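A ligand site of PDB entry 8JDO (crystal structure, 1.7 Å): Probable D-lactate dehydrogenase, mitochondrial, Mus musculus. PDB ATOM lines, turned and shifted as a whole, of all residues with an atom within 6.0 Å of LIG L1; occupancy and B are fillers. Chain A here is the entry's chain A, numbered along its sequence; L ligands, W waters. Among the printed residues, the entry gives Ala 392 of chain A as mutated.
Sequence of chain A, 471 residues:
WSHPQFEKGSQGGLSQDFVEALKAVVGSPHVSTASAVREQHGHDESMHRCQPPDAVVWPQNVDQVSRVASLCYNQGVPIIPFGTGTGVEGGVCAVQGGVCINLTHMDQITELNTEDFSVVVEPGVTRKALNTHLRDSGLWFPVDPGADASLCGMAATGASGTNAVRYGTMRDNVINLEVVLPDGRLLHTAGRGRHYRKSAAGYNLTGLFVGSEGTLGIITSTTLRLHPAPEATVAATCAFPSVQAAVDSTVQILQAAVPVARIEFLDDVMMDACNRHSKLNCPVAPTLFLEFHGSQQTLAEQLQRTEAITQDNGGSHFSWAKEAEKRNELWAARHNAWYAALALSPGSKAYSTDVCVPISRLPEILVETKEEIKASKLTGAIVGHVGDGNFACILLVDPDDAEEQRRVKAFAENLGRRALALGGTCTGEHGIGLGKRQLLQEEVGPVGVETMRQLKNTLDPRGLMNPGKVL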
ATOM      1  N   THR A  86     -12.394 -10.080  10.921  1.00  0.00           N
ATOM      2  CA  THR A  86     -11.231  -9.204  11.073  1.00  0.00           C
ATOM      3  C   THR A  86     -10.720  -8.629   9.753  1.00  0.00           C
ATOM      4  O   THR A  86      -9.699  -7.941   9.747  1.00  0.00           O
ATOM      5  CB  THR A  86     -10.082  -9.948  11.788  1.00  0.00           C
ATOM      6  OG1 THR A  86      -9.504 -10.939  10.920  1.00  0.00           O
ATOM      7  CG2 THR A  86     -10.560 -10.623  13.069  1.00  0.00           C
ATOM      8  N   VAL A  88     -10.353  -6.194   6.384  1.00  0.00           N
ATOM      9  CA  VAL A  88     -10.292  -4.746   6.370  1.00  0.00           C
ATOM     10  C   VAL A  88     -10.758  -4.121   5.055  1.00  0.00           C
ATOM     11  O   VAL A  88     -10.463  -2.952   4.799  1.00  0.00           O
ATOM     12  CB  VAL A  88      -8.870  -4.252   6.714  1.00  0.00           C
ATOM     13  CG1 VAL A  88      -8.504  -4.688   8.123  1.00  0.00           C
ATOM     14  CG2 VAL A  88      -7.862  -4.767   5.703  1.00  0.00           C
ATOM     15  N   GLY A 146      -1.875 -10.115  12.169  1.00  0.00           N
ATOM     16  CA  GLY A 146      -1.895  -9.637  13.539  1.00  0.00           C
ATOM     17  C   GLY A 146      -3.133 -10.024  14.311  1.00  0.00           C
ATOM     18  O   GLY A 146      -3.094 -10.150  15.540  1.00  0.00           O
ATOM     19  N   GLU A 264      10.257  -6.174   9.408  1.00  0.00           N
ATOM     20  CA  GLU A 264       9.062  -5.342   9.479  1.00  0.00           C
ATOM     21  C   GLU A 264       9.447  -3.889   9.662  1.00  0.00           C
ATOM     22  O   GLU A 264      10.322  -3.573  10.467  1.00  0.00           O
ATOM     23  CB  GLU A 264       8.180  -5.779  10.644  1.00  0.00           C
ATOM     24  CG  GLU A 264       7.521  -7.142  10.413  1.00  0.00           C
ATOM     25  CD  GLU A 264       6.517  -7.099   9.299  1.00  0.00           C
ATOM     26  OE1 GLU A 264       5.697  -6.163   9.317  1.00  0.00           O
ATOM     27  OE2 GLU A 264       6.477  -8.033   8.463  1.00  0.00           O
ATOM     28  N   ARG A 334       3.869  -5.427  17.414  1.00  0.00           N
ATOM     29  CA  ARG A 334       3.769  -5.325  15.959  1.00  0.00           C
ATOM     30  C   ARG A 334       2.404  -5.822  15.483  1.00  0.00           C
ATOM     31  O   ARG A 334       1.744  -5.182  14.657  1.00  0.00           O
ATOM     32  CB  ARG A 334       4.901  -6.108  15.306  1.00  0.00           C
ATOM     33  CG  ARG A 334       4.730  -6.352  13.818  1.00  0.00           C
ATOM     34  CD  ARG A 334       4.649  -5.038  13.035  1.00  0.00           C
ATOM     35  NE  ARG A 334       4.337  -5.311  11.641  1.00  0.00           N
ATOM     36  CZ  ARG A 334       3.108  -5.295  11.138  1.00  0.00           C
ATOM     37  NH1 ARG A 334       2.084  -4.999  11.937  1.00  0.00           N
ATOM     38  NH2 ARG A 334       2.910  -5.568   9.845  1.00  0.00           N
ATOM     39  N   HIS A 335       1.967  -6.974  16.008  1.00  0.00           N
ATOM     40  CA  HIS A 335       0.691  -7.541  15.556  1.00  0.00           C
ATOM     41  C   HIS A 335      -0.476  -6.622  15.890  1.00  0.00           C
ATOM     42  O   HIS A 335      -1.492  -6.623  15.193  1.00  0.00           O
ATOM     43  CB  HIS A 335       0.493  -8.918  16.178  1.00  0.00           C
ATOM     44  CG  HIS A 335       1.293 -10.001  15.518  1.00  0.00           C
ATOM     45  ND1 HIS A 335       1.800 -11.090  16.210  1.00  0.00           N
ATOM     46  CD2 HIS A 335       1.643 -10.194  14.215  1.00  0.00           C
ATOM     47  CE1 HIS A 335       2.439 -11.884  15.367  1.00  0.00           C
ATOM     48  NE2 HIS A 335       2.351 -11.374  14.158  1.00  0.00           N
ATOM     49  N   ALA A 337      -0.343  -3.303  15.821  1.00  0.00           N
ATOM     50  CA  ALA A 337      -0.102  -1.974  15.258  1.00  0.00           C
ATOM     51  C   ALA A 337      -1.378  -1.302  14.786  1.00  0.00           C
ATOM     52  O   ALA A 337      -1.559  -0.087  14.943  1.00  0.00           O
ATOM     53  CB  ALA A 337       0.908  -2.067  14.110  1.00  0.00           C
ATOM     54  N   TRP A 338      -2.292  -2.067  14.175  1.00  0.00           N
ATOM     55  CA  TRP A 338      -3.551  -1.494  13.728  1.00  0.00           C
ATOM     56  C   TRP A 338      -4.276  -0.812  14.878  1.00  0.00           C
ATOM     57  O   TRP A 338      -4.714   0.335  14.763  1.00  0.00           O
ATOM     58  CB  TRP A 338      -4.414  -2.578  13.097  1.00  0.00           C
ATOM     59  CG  TRP A 338      -5.844  -2.211  12.802  1.00  0.00           C
ATOM     60  CD1 TRP A 338      -6.949  -2.618  13.492  1.00  0.00           C
ATOM     61  CD2 TRP A 338      -6.337  -1.442  11.691  1.00  0.00           C
ATOM     62  NE1 TRP A 338      -8.095  -2.141  12.894  1.00  0.00           N
ATOM     63  CE2 TRP A 338      -7.742  -1.424  11.781  1.00  0.00           C
ATOM     64  CE3 TRP A 338      -5.717  -0.764  10.639  1.00  0.00           C
ATOM     65  CZ2 TRP A 338      -8.541  -0.722  10.878  1.00  0.00           C
ATOM     66  CZ3 TRP A 338      -6.515  -0.086   9.714  1.00  0.00           C
ATOM     67  CH2 TRP A 338      -7.912  -0.079   9.845  1.00  0.00           C
ATOM     68  N   SER A 352      -6.916   1.303   5.465  1.00  0.00           N
ATOM     69  CA  SER A 352      -5.543   0.871   5.258  1.00  0.00           C
ATOM     70  C   SER A 352      -5.302   0.635   3.787  1.00  0.00           C
ATOM     71  O   SER A 352      -6.121   0.005   3.105  1.00  0.00           O
ATOM     72  CB  SER A 352      -5.239  -0.422   6.024  1.00  0.00           C
ATOM     73  OG  SER A 352      -3.868  -0.795   5.841  1.00  0.00           O
ATOM     74  N   THR A 353      -4.180   1.137   3.286  1.00  0.00           N
ATOM     75  CA  THR A 353      -3.666   0.709   1.993  1.00  0.00           C
ATOM     76  C   THR A 353      -2.806  -0.539   2.181  1.00  0.00           C
ATOM     77  O   THR A 353      -2.527  -0.961   3.293  1.00  0.00           O
ATOM     78  CB  THR A 353      -2.861   1.845   1.345  1.00  0.00           C
ATOM     79  OG1 THR A 353      -1.692   2.097   2.130  1.00  0.00           O
ATOM     80  CG2 THR A 353      -3.692   3.108   1.264  1.00  0.00           C
ATOM     81  N   ASP A 354      -2.379  -1.128   1.060  1.00  0.00           N
ATOM     82  CA  ASP A 354      -1.734  -2.435   1.100  1.00  0.00           C
ATOM     83  C   ASP A 354      -0.913  -2.722  -0.151  1.00  0.00           C
ATOM     84  O   ASP A 354      -0.821  -3.877  -0.580  1.00  0.00           O
ATOM     85  CB  ASP A 354      -2.817  -3.530   1.264  1.00  0.00           C
ATOM     86  CG  ASP A 354      -2.243  -4.927   1.492  1.00  0.00           C
ATOM     87  OD1 ASP A 354      -1.166  -5.060   2.120  1.00  0.00           O
ATOM     88  OD2 ASP A 354      -2.887  -5.898   1.044  1.00  0.00           O
ATOM     89  N   VAL A 383       3.258   0.938   8.424  1.00  0.00           N
ATOM     90  CA  VAL A 383       3.832  -0.288   8.944  1.00  0.00           C
ATOM     91  C   VAL A 383       3.867  -1.273   7.794  1.00  0.00           C
ATOM     92  O   VAL A 383       3.041  -1.211   6.887  1.00  0.00           O
ATOM     93  CB  VAL A 383       3.020  -0.835  10.143  1.00  0.00           C
ATOM     94  CG1 VAL A 383       1.631  -1.330   9.669  1.00  0.00           C
ATOM     95  CG2 VAL A 383       3.788  -1.924  10.852  1.00  0.00           C
ATOM     96  N   GLY A 384       4.830  -2.178   7.792  1.00  0.00           N
ATOM     97  CA  GLY A 384       4.800  -2.997   6.602  1.00  0.00           C
ATOM     98  C   GLY A 384       5.661  -4.230   6.504  1.00  0.00           C
ATOM     99  O   GLY A 384       6.769  -4.283   7.031  1.00  0.00           O
ATOM    100  N   HIS A 385       5.130  -5.237   5.796  1.00  0.00           N
ATOM    101  CA  HIS A 385       5.896  -6.430   5.434  1.00  0.00           C
ATOM    102  C   HIS A 385       6.838  -6.104   4.281  1.00  0.00           C
ATOM    103  O   HIS A 385       6.696  -6.580   3.155  1.00  0.00           O
ATOM    104  CB  HIS A 385       4.960  -7.584   5.052  1.00  0.00           C
ATOM    105  CG  HIS A 385       3.822  -7.806   5.994  1.00  0.00           C
ATOM    106  ND1 HIS A 385       4.002  -8.112   7.329  1.00  0.00           N
ATOM    107  CD2 HIS A 385       2.486  -7.846   5.777  1.00  0.00           C
ATOM    108  CE1 HIS A 385       2.823  -8.303   7.899  1.00  0.00           C
ATOM    109  NE2 HIS A 385       1.878  -8.153   6.981  1.00  0.00           N
ATOM    110  N   ALA A 392       1.625  -1.031   4.539  1.00  0.00           N
ATOM    111  CA  ALA A 392       0.303  -0.491   4.802  1.00  0.00           C
ATOM    112  C   ALA A 392       0.435   0.944   5.301  1.00  0.00           C
ATOM    113  O   ALA A 392       1.282   1.231   6.152  1.00  0.00           O
ATOM    114  CB  ALA A 392      -0.446  -1.328   5.849  1.00  0.00           C
ATOM    115  N   ILE A 394      -1.896   3.392   7.326  1.00  0.00           N
ATOM    116  CA  ILE A 394      -3.107   3.386   8.148  1.00  0.00           C
ATOM    117  C   ILE A 394      -3.558   4.820   8.333  1.00  0.00           C
ATOM    118  O   ILE A 394      -2.826   5.633   8.917  1.00  0.00           O
ATOM    119  CB  ILE A 394      -2.862   2.706   9.513  1.00  0.00           C
ATOM    120  CG1 ILE A 394      -2.406   1.255   9.300  1.00  0.00           C
ATOM    121  CG2 ILE A 394      -4.135   2.808  10.365  1.00  0.00           C
ATOM    122  CD1 ILE A 394      -1.791   0.609  10.543  1.00  0.00           C
ATOM    123  N   GLU A 429      -1.961  -8.422   0.345  1.00  0.00           N
ATOM    124  CA  GLU A 429      -2.510  -9.476   1.188  1.00  0.00           C
ATOM    125  C   GLU A 429      -3.951  -9.253   1.669  1.00  0.00           C
ATOM    126  O   GLU A 429      -4.657 -10.221   1.934  1.00  0.00           O
ATOM    127  CB  GLU A 429      -1.603  -9.671   2.416  1.00  0.00           C
ATOM    128  CG  GLU A 429      -1.452  -8.370   3.239  1.00  0.00           C
ATOM    129  CD  GLU A 429      -0.646  -8.537   4.518  1.00  0.00           C
ATOM    130  OE1 GLU A 429      -0.133  -9.652   4.799  1.00  0.00           O
ATOM    131  OE2 GLU A 429      -0.568  -7.535   5.275  1.00  0.00           O
ATOM    132  N   HIS A 430      -4.399  -8.001   1.824  1.00  0.00           N
ATOM    133  CA  HIS A 430      -5.709  -7.777   2.435  1.00  0.00           C
ATOM    134  C   HIS A 430      -6.864  -8.157   1.527  1.00  0.00           C
ATOM    135  O   HIS A 430      -7.944  -8.515   2.007  1.00  0.00           O
ATOM    136  CB  HIS A 430      -5.875  -6.309   2.788  1.00  0.00           C
ATOM    137  CG  HIS A 430      -4.965  -5.848   3.869  1.00  0.00           C
ATOM    138  ND1 HIS A 430      -4.654  -4.524   4.051  1.00  0.00           N
ATOM    139  CD2 HIS A 430      -4.290  -6.541   4.821  1.00  0.00           C
ATOM    140  CE1 HIS A 430      -3.818  -4.412   5.064  1.00  0.00           C
ATOM    141  NE2 HIS A 430      -3.576  -5.619   5.553  1.00  0.00           N
HETATM  142  C1  LIG L   1      -4.624  -4.133   8.523  1.00  0.00           C
HETATM  143  C2  LIG L   1      -3.479  -3.121   8.444  1.00  0.00           C
HETATM  144  C3  LIG L   1      -0.595  -5.395   9.573  1.00  0.00           C
HETATM  145  O1  LIG L   1       0.391  -5.549   8.804  1.00  0.00           O
HETATM  146  O2  LIG L   1      -1.772  -5.382   7.556  1.00  0.00           O
HETATM  147  C4  LIG L   1      -1.921  -5.087   8.917  1.00  0.00           C
HETATM  148  O3  LIG L   1      -0.481  -5.489  10.835  1.00  0.00           O
HETATM  149  C5  LIG L   1      -2.192  -3.595   9.119  1.00  0.00           C
HETATM  150  C6  LIG L   1      -5.203  -4.215   9.937  1.00  0.00           C
HETATM  151  P1  LG2 L   2     -13.679 -12.050   7.558  1.00  0.00           P
HETATM  152  O1  LG2 L   2     -13.634 -10.576   7.722  1.00  0.00           O
HETATM  153  O2  LG2 L   2     -14.660 -12.871   8.352  1.00  0.00           O
HETATM  154  O3  LG2 L   2     -13.930 -12.310   5.989  1.00  0.00           O
HETATM  155  C1  LG2 L   2     -12.997 -11.802   5.012  1.00  0.00           C
HETATM  156  C2  LG2 L   2     -13.475 -12.139   3.617  1.00  0.00           C
HETATM  157  O4  LG2 L   2     -13.313 -13.552   3.387  1.00  0.00           O
HETATM  158  C3  LG2 L   2     -14.947 -11.844   3.350  1.00  0.00           C
HETATM  159  O5  LG2 L   2     -15.149 -11.459   1.998  1.00  0.00           O
HETATM  160  C4  LG2 L   2     -15.629 -13.170   3.693  1.00  0.00           C
HETATM  161  O6  LG2 L   2     -16.841 -13.399   2.961  1.00  0.00           O
HETATM  162  C5  LG2 L   2     -14.584 -14.176   3.230  1.00  0.00           C
HETATM  163  N1  LG2 L   2     -14.543 -15.411   3.985  1.00  0.00           N
HETATM  164  C6  LG2 L   2     -14.291 -15.567   5.324  1.00  0.00           C
HETATM  165  N2  LG2 L   2     -14.252 -16.815   5.721  1.00  0.00           N
HETATM  166  C7  LG2 L   2     -14.501 -17.541   4.566  1.00  0.00           C
HETATM  167  C8  LG2 L   2     -14.615 -18.916   4.328  1.00  0.00           C
HETATM  168  N3  LG2 L   2     -14.456 -19.851   5.269  1.00  0.00           N
HETATM  169  N4  LG2 L   2     -14.885 -19.302   3.051  1.00  0.00           N
HETATM  170  C9  LG2 L   2     -15.044 -18.367   2.111  1.00  0.00           C
HETATM  171  N5  LG2 L   2     -14.950 -17.045   2.228  1.00  0.00           N
HETATM  172  C10 LG2 L   2     -14.684 -16.688   3.490  1.00  0.00           C
HETATM  173  N6  LG2 L   2      -4.279  -9.597   6.919  1.00  0.00           N
HETATM  174  C11 LG2 L   2      -3.135 -10.007   6.301  1.00  0.00           C
HETATM  175  O7  LG2 L   2      -3.160 -10.574   5.210  1.00  0.00           O
HETATM  176  N7  LG2 L   2      -1.907  -9.791   6.911  1.00  0.00           N
HETATM  177  C12 LG2 L   2      -1.707  -9.196   8.139  1.00  0.00           C
HETATM  178  O8  LG2 L   2      -0.561  -9.047   8.574  1.00  0.00           O
HETATM  179  C13 LG2 L   2      -2.929  -8.762   8.788  1.00  0.00           C
HETATM  180  N8  LG2 L   2      -2.842  -8.182   9.990  1.00  0.00           N
HETATM  181  C14 LG2 L   2      -4.012  -7.771  10.592  1.00  0.00           C
HETATM  182  C15 LG2 L   2      -3.937  -7.170  11.851  1.00  0.00           C
HETATM  183  C16 LG2 L   2      -5.090  -6.749  12.503  1.00  0.00           C
HETATM  184  C17 LG2 L   2      -4.974  -6.078  13.851  1.00  0.00           C
HETATM  185  C18 LG2 L   2      -6.343  -6.927  11.897  1.00  0.00           C
HETATM  186  C19 LG2 L   2      -7.614  -6.465  12.571  1.00  0.00           C
HETATM  187  C20 LG2 L   2      -6.423  -7.534  10.645  1.00  0.00           C
HETATM  188  C21 LG2 L   2      -5.274  -7.961   9.999  1.00  0.00           C
HETATM  189  N9  LG2 L   2      -5.328  -8.607   8.743  1.00  0.00           N
HETATM  190  C22 LG2 L   2      -4.168  -9.006   8.100  1.00  0.00           C
HETATM  191  C23 LG2 L   2      -6.605  -8.744   8.025  1.00  0.00           C
HETATM  192  C24 LG2 L   2      -7.421  -9.978   8.381  1.00  0.00           C
HETATM  193  O9  LG2 L   2      -7.067 -10.430   9.693  1.00  0.00           O
HETATM  194  C25 LG2 L   2      -7.183 -11.044   7.317  1.00  0.00           C
HETATM  195  O10 LG2 L   2      -7.663 -10.538   6.078  1.00  0.00           O
HETATM  196  C26 LG2 L   2      -7.886 -12.363   7.637  1.00  0.00           C
HETATM  197  O11 LG2 L   2      -7.498 -13.315   6.640  1.00  0.00           O
HETATM  198  C27 LG2 L   2      -9.391 -12.215   7.664  1.00  0.00           C
HETATM  199  O12 LG2 L   2      -9.971 -13.434   8.171  1.00  0.00           O
HETATM  200  P2  LG2 L   2     -11.404 -13.410   8.820  1.00  0.00           P
HETATM  201  O13 LG2 L   2     -11.935 -14.828   9.010  1.00  0.00           O
HETATM  202  O14 LG2 L   2     -11.380 -12.576  10.079  1.00  0.00           O
HETATM  203  O15 LG2 L   2     -12.216 -12.652   7.674  1.00  0.00           O
HETATM  204  O   HOH W   1      -0.255  -5.038   4.688  1.00  0.00           O
HETATM  205  O   HOH W   2      -1.662  -4.627  13.058  1.00  0.00           O
HETATM  206  O   HOH W   3       0.408  -7.917  12.030  1.00  0.00           O
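A ring nitrogen (NE2) of His 430 is in hydrogen-bond range of an oxygen (O2) of LIG L1 (2.7 Å).
NH2 of Arg 334 lies within salt-bridge range of O1 of LIG L1 (2.7 Å).
OE2 of Glu 429 sits at hydrogen-bond distance from O2 of LIG L1 (3.4 Å).
OE1 of Glu 429 lies within hydrogen-bond range of N7 of LG2 L2 (2.8 Å).
A ring nitrogen (NE2) of His 385 lies within hydrogen-bond range of an oxygen (O8) of LG2 L2, 3.0 Å away.
N of Gly 146 is in hydrogen-bond range of N8 of LG2 L2, 3.1 Å away.
N of Thr 86 sits at hydrogen-bond distance from O14 of LG2 L2 (2.8 Å).
O14 of LG2 L2 is in hydrogen-bond range of OG1 of Thr 86 (2.6 Å).
The backbone NH of His 430 is in hydrogen-bond range of the side-chain carboxylate of Asp 354 (2.7 Å).
NE of Arg 334 is in salt-bridge range of OE1 of Glu 264.
OE2 of Glu 429 lies within hydrogen-bond range of NE2 of His 385, 3.0 Å away.
N of Glu 429 is in hydrogen-bond range of OD2 of Asp 354 (2.8 Å).
A ring nitrogen (ND1) of His 385 lies within hydrogen-bond range of the side-chain carboxylate of Glu 264 (2.7 Å).
Residues that only touch LIG L1: Val 88 (3.8 Å), Trp 338 (3.5 Å), Ser 352 (3.5 Å) and His 385 (3.5 Å).
Hydrophobic or aromatic side chains that line LIG L1: Val 88, Trp 338, His 385 and His 430.
Within 4 Å of LIG L1: Val 88, Arg 334, Trp 338, Ser 352, His 385, Glu 429 and His 430.
The nearest printed residue that does not touch LIG L1 is Ala 392 (4.3 Å).
Water W2 lies within hydrogen-bond range of O3 of LIG L1 (2.7 Å), N of Trp 338 (2.9 Å), O of His 335 (2.9 Å) and N of Ala 337 (3.3 Å).
Water W3 lies within hydrogen-bond range of an oxygen (O3) of LIG L1 (2.8 Å), the backbone NH of Gly 146 (3.2 Å) and the guanidinium group of Arg 334 (3.4 Å).
Water W1 lies within hydrogen-bond range of OE2 of Glu 429 (2.6 Å), OD1 of Asp 354 (2.7 Å), O2 of LIG L1 (3.3 Å) and NE2 of His 430 (3.5 Å).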
